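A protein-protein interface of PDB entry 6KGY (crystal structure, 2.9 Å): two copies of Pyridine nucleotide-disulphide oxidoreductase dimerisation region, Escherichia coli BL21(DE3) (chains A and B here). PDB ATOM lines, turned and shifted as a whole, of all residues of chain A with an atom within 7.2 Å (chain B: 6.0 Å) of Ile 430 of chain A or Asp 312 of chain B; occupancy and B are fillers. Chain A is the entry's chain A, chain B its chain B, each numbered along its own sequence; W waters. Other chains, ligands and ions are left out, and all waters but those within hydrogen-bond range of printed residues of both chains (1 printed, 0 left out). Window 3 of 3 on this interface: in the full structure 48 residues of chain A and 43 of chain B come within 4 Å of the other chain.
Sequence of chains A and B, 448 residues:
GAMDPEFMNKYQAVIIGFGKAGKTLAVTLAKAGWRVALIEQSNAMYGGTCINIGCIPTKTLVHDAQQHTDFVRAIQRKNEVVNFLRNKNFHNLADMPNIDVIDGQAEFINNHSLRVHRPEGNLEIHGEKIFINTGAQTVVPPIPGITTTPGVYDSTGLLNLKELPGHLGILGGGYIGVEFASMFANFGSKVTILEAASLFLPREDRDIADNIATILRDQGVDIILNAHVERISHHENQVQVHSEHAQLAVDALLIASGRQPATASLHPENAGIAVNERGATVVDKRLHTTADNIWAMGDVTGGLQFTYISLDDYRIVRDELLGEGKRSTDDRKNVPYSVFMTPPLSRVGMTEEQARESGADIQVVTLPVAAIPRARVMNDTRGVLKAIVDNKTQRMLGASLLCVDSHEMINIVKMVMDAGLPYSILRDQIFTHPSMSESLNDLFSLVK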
ATOM      1  N   ILE A 425     -23.554  30.428   9.573  1.00  0.00           N
ATOM      2  CA  ILE A 425     -23.114  29.828  10.826  1.00  0.00           C
ATOM      3  C   ILE A 425     -24.266  29.745  11.816  1.00  0.00           C
ATOM      4  O   ILE A 425     -24.505  28.697  12.424  1.00  0.00           O
ATOM      5  CB  ILE A 425     -21.916  30.603  11.401  1.00  0.00           C
ATOM      6  CG1 ILE A 425     -20.722  30.458  10.453  1.00  0.00           C
ATOM      7  CG2 ILE A 425     -21.590  30.124  12.812  1.00  0.00           C
ATOM      8  CD1 ILE A 425     -19.371  30.582  11.124  1.00  0.00           C
ATOM      9  N   LEU A 426     -25.011  30.841  11.981  1.00  0.00           N
ATOM     10  CA  LEU A 426     -26.174  30.820  12.860  1.00  0.00           C
ATOM     11  C   LEU A 426     -27.316  29.996  12.280  1.00  0.00           C
ATOM     12  O   LEU A 426     -28.199  29.565  13.029  1.00  0.00           O
ATOM     13  CB  LEU A 426     -26.640  32.249  13.138  1.00  0.00           C
ATOM     14  CG  LEU A 426     -25.562  33.150  13.739  1.00  0.00           C
ATOM     15  CD1 LEU A 426     -26.146  34.481  14.184  1.00  0.00           C
ATOM     16  CD2 LEU A 426     -24.889  32.444  14.897  1.00  0.00           C
ATOM     17  N   ARG A 427     -27.314  29.768  10.967  1.00  0.00           N
ATOM     18  CA  ARG A 427     -28.329  28.924  10.350  1.00  0.00           C
ATOM     19  C   ARG A 427     -28.141  27.456  10.714  1.00  0.00           C
ATOM     20  O   ARG A 427     -29.126  26.722  10.854  1.00  0.00           O
ATOM     21  CB  ARG A 427     -28.291  29.109   8.833  1.00  0.00           C
ATOM     22  CG  ARG A 427     -29.347  28.344   8.059  1.00  0.00           C
ATOM     23  CD  ARG A 427     -28.946  28.235   6.597  1.00  0.00           C
ATOM     24  NE  ARG A 427     -27.712  27.468   6.441  1.00  0.00           N
ATOM     25  CZ  ARG A 427     -26.919  27.525   5.375  1.00  0.00           C
ATOM     26  NH1 ARG A 427     -27.221  28.322   4.360  1.00  0.00           N
ATOM     27  NH2 ARG A 427     -25.818  26.788   5.327  1.00  0.00           N
ATOM     28  N   ASP A 428     -26.894  27.013  10.883  1.00  0.00           N
ATOM     29  CA  ASP A 428     -26.582  25.608  11.112  1.00  0.00           C
ATOM     30  C   ASP A 428     -25.998  25.332  12.491  1.00  0.00           C
ATOM     31  O   ASP A 428     -25.715  24.171  12.805  1.00  0.00           O
ATOM     32  CB  ASP A 428     -25.608  25.111  10.036  1.00  0.00           C
ATOM     33  CG  ASP A 428     -26.017  25.532   8.635  1.00  0.00           C
ATOM     34  OD1 ASP A 428     -25.120  25.766   7.798  1.00  0.00           O
ATOM     35  OD2 ASP A 428     -27.233  25.628   8.369  1.00  0.00           O
ATOM     36  N   GLN A 429     -25.809  26.354  13.322  1.00  0.00           N
ATOM     37  CA  GLN A 429     -25.214  26.144  14.633  1.00  0.00           C
ATOM     38  C   GLN A 429     -26.216  25.484  15.575  1.00  0.00           C
ATOM     39  O   GLN A 429     -27.425  25.723  15.502  1.00  0.00           O
ATOM     40  CB  GLN A 429     -24.721  27.471  15.213  1.00  0.00           C
ATOM     41  CG  GLN A 429     -25.003  27.683  16.687  1.00  0.00           C
ATOM     42  CD  GLN A 429     -23.736  27.775  17.512  1.00  0.00           C
ATOM     43  OE1 GLN A 429     -22.631  27.841  16.972  1.00  0.00           O
ATOM     44  NE2 GLN A 429     -23.890  27.788  18.829  1.00  0.00           N
ATOM     45  N   ILE A 430     -25.699  24.636  16.458  1.00  0.00           N
ATOM     46  CA  ILE A 430     -26.518  23.900  17.413  1.00  0.00           C
ATOM     47  C   ILE A 430     -26.680  24.759  18.662  1.00  0.00           C
ATOM     48  O   ILE A 430     -25.734  24.926  19.437  1.00  0.00           O
ATOM     49  CB  ILE A 430     -25.895  22.542  17.754  1.00  0.00           C
ATOM     50  CG1 ILE A 430     -25.773  21.670  16.503  1.00  0.00           C
ATOM     51  CG2 ILE A 430     -26.713  21.834  18.815  1.00  0.00           C
ATOM     52  CD1 ILE A 430     -24.824  20.497  16.676  1.00  0.00           C
ATOM     53  N   PHE A 431     -27.877  25.304  18.860  1.00  0.00           N
ATOM     54  CA  PHE A 431     -28.205  26.063  20.055  1.00  0.00           C
ATOM     55  C   PHE A 431     -28.863  25.154  21.088  1.00  0.00           C
ATOM     56  O   PHE A 431     -29.289  24.034  20.792  1.00  0.00           O
ATOM     57  CB  PHE A 431     -29.128  27.239  19.719  1.00  0.00           C
ATOM     58  CG  PHE A 431     -28.453  28.342  18.958  1.00  0.00           C
ATOM     59  CD1 PHE A 431     -27.657  29.269  19.611  1.00  0.00           C
ATOM     60  CD2 PHE A 431     -28.617  28.454  17.587  1.00  0.00           C
ATOM     61  CE1 PHE A 431     -27.028  30.283  18.908  1.00  0.00           C
ATOM     62  CE2 PHE A 431     -27.994  29.468  16.880  1.00  0.00           C
ATOM     63  CZ  PHE A 431     -27.198  30.382  17.542  1.00  0.00           C
ATOM     64  N   THR A 432     -28.935  25.649  22.319  1.00  0.00           N
ATOM     65  CA  THR A 432     -29.665  24.940  23.355  1.00  0.00           C
ATOM     66  C   THR A 432     -31.165  25.027  23.090  1.00  0.00           C
ATOM     67  O   THR A 432     -31.642  25.869  22.325  1.00  0.00           O
ATOM     68  CB  THR A 432     -29.336  25.506  24.736  1.00  0.00           C
ATOM     69  OG1 THR A 432     -29.187  26.928  24.652  1.00  0.00           O
ATOM     70  CG2 THR A 432     -28.047  24.894  25.263  1.00  0.00           C
ATOM     71  N   GLU A 438     -32.026  30.129  19.743  1.00  0.00           N
ATOM     72  CA  GLU A 438     -32.173  29.127  18.695  1.00  0.00           C
ATOM     73  C   GLU A 438     -33.160  29.548  17.615  1.00  0.00           C
ATOM     74  O   GLU A 438     -33.258  28.859  16.594  1.00  0.00           O
ATOM     75  CB  GLU A 438     -32.601  27.788  19.295  1.00  0.00           C
ATOM     76  CG  GLU A 438     -34.019  27.756  19.821  1.00  0.00           C
ATOM     77  CD  GLU A 438     -34.430  26.371  20.274  1.00  0.00           C
ATOM     78  OE1 GLU A 438     -35.297  26.269  21.167  1.00  0.00           O
ATOM     79  OE2 GLU A 438     -33.886  25.384  19.737  1.00  0.00           O
ATOM     80  N   ASN A 441     -31.732  29.816  14.154  1.00  0.00           N
ATOM     81  CA  ASN A 441     -31.800  28.673  13.249  1.00  0.00           C
ATOM     82  C   ASN A 441     -32.878  28.893  12.196  1.00  0.00           C
ATOM     83  O   ASN A 441     -32.644  28.703  10.997  1.00  0.00           O
ATOM     84  CB  ASN A 441     -32.082  27.390  14.037  1.00  0.00           C
ATOM     85  CG  ASN A 441     -30.828  26.767  14.617  1.00  0.00           C
ATOM     86  OD1 ASN A 441     -29.723  26.989  14.123  1.00  0.00           O
ATOM     87  ND2 ASN A 441     -30.994  25.976  15.671  1.00  0.00           N
ATOM     88  N   LEU B 287     -26.150   8.311   9.613  1.00  0.00           N
ATOM     89  CA  LEU B 287     -27.415   7.815  10.149  1.00  0.00           C
ATOM     90  C   LEU B 287     -28.051   6.732   9.287  1.00  0.00           C
ATOM     91  O   LEU B 287     -29.272   6.546   9.326  1.00  0.00           O
ATOM     92  CB  LEU B 287     -28.407   8.962  10.373  1.00  0.00           C
ATOM     93  CG  LEU B 287     -27.807  10.157  11.117  1.00  0.00           C
ATOM     94  CD1 LEU B 287     -28.731  11.348  11.034  1.00  0.00           C
ATOM     95  CD2 LEU B 287     -27.507   9.797  12.563  1.00  0.00           C
ATOM     96  N   THR B 307     -33.395  17.783  21.607  1.00  0.00           N
ATOM     97  CA  THR B 307     -34.122  18.177  20.406  1.00  0.00           C
ATOM     98  C   THR B 307     -33.191  18.775  19.356  1.00  0.00           C
ATOM     99  O   THR B 307     -33.415  18.592  18.154  1.00  0.00           O
ATOM    100  CB  THR B 307     -35.234  19.164  20.775  1.00  0.00           C
ATOM    101  OG1 THR B 307     -36.167  18.523  21.653  1.00  0.00           O
ATOM    102  CG2 THR B 307     -35.974  19.641  19.537  1.00  0.00           C
ATOM    103  N   TYR B 308     -32.132  19.468  19.784  1.00  0.00           N
ATOM    104  CA  TYR B 308     -31.224  20.080  18.819  1.00  0.00           C
ATOM    105  C   TYR B 308     -30.323  19.047  18.155  1.00  0.00           C
ATOM    106  O   TYR B 308     -29.900  19.243  17.010  1.00  0.00           O
ATOM    107  CB  TYR B 308     -30.385  21.170  19.488  1.00  0.00           C
ATOM    108  CG  TYR B 308     -29.859  20.827  20.864  1.00  0.00           C
ATOM    109  CD1 TYR B 308     -28.666  20.133  21.020  1.00  0.00           C
ATOM    110  CD2 TYR B 308     -30.541  21.221  22.009  1.00  0.00           C
ATOM    111  CE1 TYR B 308     -28.173  19.830  22.275  1.00  0.00           C
ATOM    112  CE2 TYR B 308     -30.057  20.920  23.269  1.00  0.00           C
ATOM    113  CZ  TYR B 308     -28.872  20.226  23.396  1.00  0.00           C
ATOM    114  OH  TYR B 308     -28.390  19.926  24.649  1.00  0.00           O
ATOM    115  N   ILE B 309     -30.012  17.951  18.850  1.00  0.00           N
ATOM    116  CA  ILE B 309     -29.259  16.873  18.215  1.00  0.00           C
ATOM    117  C   ILE B 309     -30.134  16.146  17.202  1.00  0.00           C
ATOM    118  O   ILE B 309     -29.666  15.745  16.128  1.00  0.00           O
ATOM    119  CB  ILE B 309     -28.696  15.913  19.280  1.00  0.00           C
ATOM    120  CG1 ILE B 309     -27.589  16.599  20.084  1.00  0.00           C
ATOM    121  CG2 ILE B 309     -28.167  14.639  18.636  1.00  0.00           C
ATOM    122  CD1 ILE B 309     -26.646  17.439  19.244  1.00  0.00           C
ATOM    123  N   SER B 310     -31.420  15.979  17.518  1.00  0.00           N
ATOM    124  CA  SER B 310     -32.345  15.370  16.567  1.00  0.00           C
ATOM    125  C   SER B 310     -32.471  16.215  15.306  1.00  0.00           C
ATOM    126  O   SER B 310     -32.577  15.677  14.198  1.00  0.00           O
ATOM    127  CB  SER B 310     -33.711  15.171  17.221  1.00  0.00           C
ATOM    128  OG  SER B 310     -34.526  14.308  16.446  1.00  0.00           O
ATOM    129  N   LEU B 311     -32.455  17.543  15.452  1.00  0.00           N
ATOM    130  CA  LEU B 311     -32.514  18.408  14.279  1.00  0.00           C
ATOM    131  C   LEU B 311     -31.189  18.408  13.524  1.00  0.00           C
ATOM    132  O   LEU B 311     -31.177  18.552  12.297  1.00  0.00           O
ATOM    133  CB  LEU B 311     -32.920  19.825  14.693  1.00  0.00           C
ATOM    134  CG  LEU B 311     -32.515  21.055  13.872  1.00  0.00           C
ATOM    135  CD1 LEU B 311     -33.101  21.024  12.467  1.00  0.00           C
ATOM    136  CD2 LEU B 311     -32.966  22.316  14.594  1.00  0.00           C
ATOM    137  N   ASP B 312     -30.067  18.235  14.228  1.00  0.00           N
ATOM    138  CA  ASP B 312     -28.797  18.054  13.532  1.00  0.00           C
ATOM    139  C   ASP B 312     -28.794  16.752  12.742  1.00  0.00           C
ATOM    140  O   ASP B 312     -28.195  16.676  11.663  1.00  0.00           O
ATOM    141  CB  ASP B 312     -27.633  18.086  14.522  1.00  0.00           C
ATOM    142  CG  ASP B 312     -26.291  18.240  13.831  1.00  0.00           C
ATOM    143  OD1 ASP B 312     -26.119  19.223  13.080  1.00  0.00           O
ATOM    144  OD2 ASP B 312     -25.410  17.377  14.031  1.00  0.00           O
ATOM    145  N   ASP B 313     -29.454  15.717  13.271  1.00  0.00           N
ATOM    146  CA  ASP B 313     -29.653  14.492  12.506  1.00  0.00           C
ATOM    147  C   ASP B 313     -30.334  14.784  11.177  1.00  0.00           C
ATOM    148  O   ASP B 313     -29.984  14.199  10.146  1.00  0.00           O
ATOM    149  CB  ASP B 313     -30.484  13.493  13.316  1.00  0.00           C
ATOM    150  CG  ASP B 313     -29.643  12.650  14.252  1.00  0.00           C
ATOM    151  OD1 ASP B 313     -28.410  12.592  14.061  1.00  0.00           O
ATOM    152  OD2 ASP B 313     -30.217  12.043  15.181  1.00  0.00           O
ATOM    153  N   TYR B 314     -31.311  15.695  11.184  1.00  0.00           N
ATOM    154  CA  TYR B 314     -31.980  16.076   9.944  1.00  0.00           C
ATOM    155  C   TYR B 314     -31.003  16.711   8.962  1.00  0.00           C
ATOM    156  O   TYR B 314     -31.024  16.397   7.766  1.00  0.00           O
ATOM    157  CB  TYR B 314     -33.132  17.036  10.243  1.00  0.00           C
ATOM    158  CG  TYR B 314     -33.366  18.060   9.154  1.00  0.00           C
ATOM    159  CD1 TYR B 314     -33.994  17.707   7.968  1.00  0.00           C
ATOM    160  CD2 TYR B 314     -32.950  19.376   9.310  1.00  0.00           C
ATOM    161  CE1 TYR B 314     -34.206  18.637   6.968  1.00  0.00           C
ATOM    162  CE2 TYR B 314     -33.158  20.313   8.315  1.00  0.00           C
ATOM    163  CZ  TYR B 314     -33.786  19.938   7.146  1.00  0.00           C
ATOM    164  OH  TYR B 314     -33.997  20.865   6.151  1.00  0.00           O
ATOM    165  N   ARG B 315     -30.144  17.612   9.449  1.00  0.00           N
ATOM    166  CA  ARG B 315     -29.160  18.250   8.580  1.00  0.00           C
ATOM    167  C   ARG B 315     -28.293  17.215   7.876  1.00  0.00           C
ATOM    168  O   ARG B 315     -27.905  17.403   6.717  1.00  0.00           O
ATOM    169  CB  ARG B 315     -28.285  19.208   9.390  1.00  0.00           C
ATOM    170  CG  ARG B 315     -28.959  20.514   9.774  1.00  0.00           C
ATOM    171  CD  ARG B 315     -28.019  21.394  10.585  1.00  0.00           C
ATOM    172  NE  ARG B 315     -28.736  22.448  11.297  1.00  0.00           N
ATOM    173  CZ  ARG B 315     -28.763  22.573  12.620  1.00  0.00           C
ATOM    174  NH1 ARG B 315     -28.110  21.706  13.384  1.00  0.00           N
ATOM    175  NH2 ARG B 315     -29.443  23.564  13.182  1.00  0.00           N
ATOM    176  N   ILE B 316     -27.990  16.112   8.558  1.00  0.00           N
ATOM    177  CA  ILE B 316     -27.120  15.092   7.981  1.00  0.00           C
ATOM    178  C   ILE B 316     -27.832  14.358   6.851  1.00  0.00           C
ATOM    179  O   ILE B 316     -27.259  14.139   5.776  1.00  0.00           O
ATOM    180  CB  ILE B 316     -26.640  14.123   9.077  1.00  0.00           C
ATOM    181  CG1 ILE B 316     -25.581  14.799   9.947  1.00  0.00           C
ATOM    182  CG2 ILE B 316     -26.086  12.856   8.464  1.00  0.00           C
ATOM    183  CD1 ILE B 316     -25.465  14.212  11.330  1.00  0.00           C
ATOM    184  N   VAL B 317     -29.092  13.975   7.067  1.00  0.00           N
ATOM    185  CA  VAL B 317     -29.811  13.245   6.028  1.00  0.00           C
ATOM    186  C   VAL B 317     -30.295  14.185   4.927  1.00  0.00           C
ATOM    187  O   VAL B 317     -30.418  13.771   3.769  1.00  0.00           O
ATOM    188  CB  VAL B 317     -30.970  12.433   6.633  1.00  0.00           C
ATOM    189  CG1 VAL B 317     -30.510  11.704   7.882  1.00  0.00           C
ATOM    190  CG2 VAL B 317     -32.163  13.325   6.943  1.00  0.00           C
ATOM    191  N   ARG B 327     -22.352  15.448   4.939  1.00  0.00           N
ATOM    192  CA  ARG B 327     -21.852  15.714   6.281  1.00  0.00           C
ATOM    193  C   ARG B 327     -22.249  14.558   7.194  1.00  0.00           C
ATOM    194  O   ARG B 327     -22.982  13.650   6.795  1.00  0.00           O
ATOM    195  CB  ARG B 327     -22.383  17.047   6.824  1.00  0.00           C
ATOM    196  CG  ARG B 327     -23.897  17.153   6.875  1.00  0.00           C
ATOM    197  CD  ARG B 327     -24.335  18.479   7.482  1.00  0.00           C
ATOM    198  NE  ARG B 327     -23.425  18.935   8.528  1.00  0.00           N
ATOM    199  CZ  ARG B 327     -23.575  18.662   9.820  1.00  0.00           C
ATOM    200  NH1 ARG B 327     -24.603  17.933  10.230  1.00  0.00           N
ATOM    201  NH2 ARG B 327     -22.699  19.120  10.703  1.00  0.00           N
ATOM    202  N   SER B 328     -21.763  14.586   8.434  1.00  0.00           N
ATOM    203  CA  SER B 328     -21.905  13.427   9.305  1.00  0.00           C
ATOM    204  C   SER B 328     -21.964  13.868  10.764  1.00  0.00           C
ATOM    205  O   SER B 328     -21.798  15.046  11.090  1.00  0.00           O
ATOM    206  CB  SER B 328     -20.757  12.441   9.077  1.00  0.00           C
ATOM    207  OG  SER B 328     -19.663  12.728   9.932  1.00  0.00           O
ATOM    208  N   THR B 329     -22.212  12.892  11.647  1.00  0.00           N
ATOM    209  CA  THR B 329     -22.173  13.108  13.090  1.00  0.00           C
ATOM    210  C   THR B 329     -20.766  13.378  13.605  1.00  0.00           C
ATOM    211  O   THR B 329     -20.621  13.828  14.748  1.00  0.00           O
ATOM    212  CB  THR B 329     -22.750  11.897  13.832  1.00  0.00           C
ATOM    213  OG1 THR B 329     -21.884  10.769  13.662  1.00  0.00           O
ATOM    214  CG2 THR B 329     -24.133  11.547  13.307  1.00  0.00           C
ATOM    215  N   ARG B 332     -19.654  16.992  15.010  1.00  0.00           N
ATOM    216  CA  ARG B 332     -20.110  17.519  16.289  1.00  0.00           C
ATOM    217  C   ARG B 332     -18.946  17.704  17.252  1.00  0.00           C
ATOM    218  O   ARG B 332     -18.101  16.817  17.401  1.00  0.00           O
ATOM    219  CB  ARG B 332     -21.154  16.587  16.902  1.00  0.00           C
ATOM    220  CG  ARG B 332     -22.282  16.239  15.957  1.00  0.00           C
ATOM    221  CD  ARG B 332     -23.324  15.368  16.628  1.00  0.00           C
ATOM    222  NE  ARG B 332     -24.600  15.428  15.923  1.00  0.00           N
ATOM    223  CZ  ARG B 332     -25.537  14.489  15.991  1.00  0.00           C
ATOM    224  NH1 ARG B 332     -25.343  13.410  16.737  1.00  0.00           N
ATOM    225  NH2 ARG B 332     -26.667  14.630  15.312  1.00  0.00           N
ATOM    226  N   VAL B 335     -20.786  20.068  22.271  1.00  0.00           N
ATOM    227  CA  VAL B 335     -22.246  20.087  22.290  1.00  0.00           C
ATOM    228  C   VAL B 335     -22.706  20.638  23.634  1.00  0.00           C
ATOM    229  O   VAL B 335     -22.345  20.089  24.686  1.00  0.00           O
ATOM    230  CB  VAL B 335     -22.833  18.692  22.023  1.00  0.00           C
ATOM    231  CG1 VAL B 335     -24.299  18.652  22.426  1.00  0.00           C
ATOM    232  CG2 VAL B 335     -22.672  18.323  20.556  1.00  0.00           C
ATOM    233  N   PRO B 336     -23.486  21.715  23.652  1.00  0.00           N
ATOM    234  CA  PRO B 336     -23.932  22.296  24.917  1.00  0.00           C
ATOM    235  C   PRO B 336     -25.221  21.652  25.410  1.00  0.00           C
ATOM    236  O   PRO B 336     -25.932  20.966  24.674  1.00  0.00           O
ATOM    237  CB  PRO B 336     -24.166  23.766  24.545  1.00  0.00           C
ATOM    238  CG  PRO B 336     -24.645  23.692  23.121  1.00  0.00           C
ATOM    239  CD  PRO B 336     -24.024  22.450  22.494  1.00  0.00           C
ATOM    240  N   ASN B 411     -24.466  29.687  24.610  1.00  0.00           N
ATOM    241  CA  ASN B 411     -24.318  29.678  23.161  1.00  0.00           C
ATOM    242  C   ASN B 411     -23.235  30.643  22.698  1.00  0.00           C
ATOM    243  O   ASN B 411     -22.576  30.387  21.683  1.00  0.00           O
ATOM    244  CB  ASN B 411     -25.655  30.012  22.504  1.00  0.00           C
ATOM    245  CG  ASN B 411     -26.809  29.253  23.126  1.00  0.00           C
ATOM    246  OD1 ASN B 411     -27.781  29.847  23.592  1.00  0.00           O
ATOM    247  ND2 ASN B 411     -26.704  27.929  23.143  1.00  0.00           N
ATOM    248  N   LYS B 414     -20.095  28.569  23.299  1.00  0.00           N
ATOM    249  CA  LYS B 414     -19.915  27.501  22.321  1.00  0.00           C
ATOM    250  C   LYS B 414     -19.530  28.043  20.950  1.00  0.00           C
ATOM    251  O   LYS B 414     -18.861  27.347  20.177  1.00  0.00           O
ATOM    252  CB  LYS B 414     -21.189  26.662  22.219  1.00  0.00           C
ATOM    253  CG  LYS B 414     -21.022  25.385  21.413  1.00  0.00           C
ATOM    254  CD  LYS B 414     -22.297  25.030  20.671  1.00  0.00           C
ATOM    255  CE  LYS B 414     -22.031  24.014  19.575  1.00  0.00           C
ATOM    256  NZ  LYS B 414     -21.302  24.623  18.431  1.00  0.00           N
HETATM  257  O   HOH W   1     -22.460  23.870  15.538  1.00  0.00           O
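Arg 427 of chain A touches Arg 315 of chain B.
O of Gln 429 of chain A touches NH2 of Arg 315 of chain B, 3.8 Å away.
Gln 429 of chain A touches Lys 414 of chain B (NE2 to CD, 3.7 Å).
CG2 of Ile 430 of chain A touches CD1 of Tyr 308 of chain B, at 3.4 Å.
Asp 312 of chain B touches Ile 430 of chain A (CG to CD1, 3.9 Å).
CG1 of Ile 430 of chain A touches NH1 of Arg 315 of chain B (3.9 Å).
CD of Lys 414 of chain B touches O of Ile 430 of chain A, 3.7 Å away.
Phe 431 of chain A touches Tyr 308 of chain B (O to CG, 3.3 Å).
Asn 411 of chain B touches Phe 431 of chain A (CB to CD1, 3.6 Å).
Asn 441 of chain A touches Arg 315 of chain B (OD1 to NH2, 3.6 Å).
Of chain B, only Tyr 308, Asp 312, Arg 315 and Lys 414 come within 4 Å of Ile 430 of chain A.
Asp 312 of chain B touches just one residue of chain A: Ile 430 (3.9 Å).
Printed residues of chain B within 4 Å of Asp 428 of chain A: Arg 315 (3.4 Å).
Printed residues of chain B within 4 Å of Thr 432 of chain A: Asn 411.
Printed residues of chain B within 4 Å of Phe 431 of chain A: Tyr 308 and Asn 411.
Printed residues of chain A within 4 Å of Tyr 308 of chain B: Ile 430 and Phe 431.
Leu 426 of chain A touches none of the printed residues of chain B.
Ser 310 of chain B touches none of the printed residues of chain A.
The nearest residue of chain B that does not touch Ile 430 of chain A is Pro 336 of chain B (4.03 Å).
The nearest printed residue of chain B that does not touch Gln 429 of chain A is Asn 411 of chain B (4.1 Å).
No position is printed for both chains.
The side-chain amide oxygen (OD1) of Asn 441 of chain A lies close to the backbone carbonyl oxygen (O) of Leu 426 of chain A, 3.2 Å away.
The backbone carbonyl oxygen of Arg 427 of chain A lies close to the side-chain amide oxygen of Asn 441 of chain A (3.3 Å).
The backbone carbonyl oxygen (O) of Gln 429 of chain A lies close to the side-chain amide oxygen (OD1) of Asn 441 of chain A (3.0 Å).
The side-chain hydroxyl of Tyr 308 of chain B is in hydrogen-bond range of the backbone carbonyl oxygen of Pro 336 of chain B, at 2.7 Å.
OD1 of Asp 312 of chain B is in salt-bridge range of NH1 of Arg 315 of chain B (3.2 Å).
The side-chain carboxylate (OD2) of Asp 312 of chain B lies within salt-bridge range of the guanidinium group (NE) of Arg 332 of chain B.
Of the 20 printed residues of chain B, 5 touch a printed residue of chain A.
Along chain B the printed residues that touch a printed residue of chain A span positions 308 to 414.
Hydrophobic or aromatic side chains of chain A within 4 Å of the printed part of chain B: Ile 430 and Phe 431.
Among the printed residues, no Asp or Glu carboxylate lies within 4 Å of a Lys or Arg side-chain nitrogen of the other chain.
NH1 of Arg 315 of chain B lies close to O of Asp 428 of chain A, at 3.5 Å.
The side-chain hydroxyl (OG1) of Thr 432 of chain A sits at hydrogen-bond distance from the side-chain amide nitrogen (ND2) of Asn 411 of chain B.
Water W1 lies within hydrogen-bond range of NZ of Lys 414 of chain B and N of Ile 430 of chain A.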
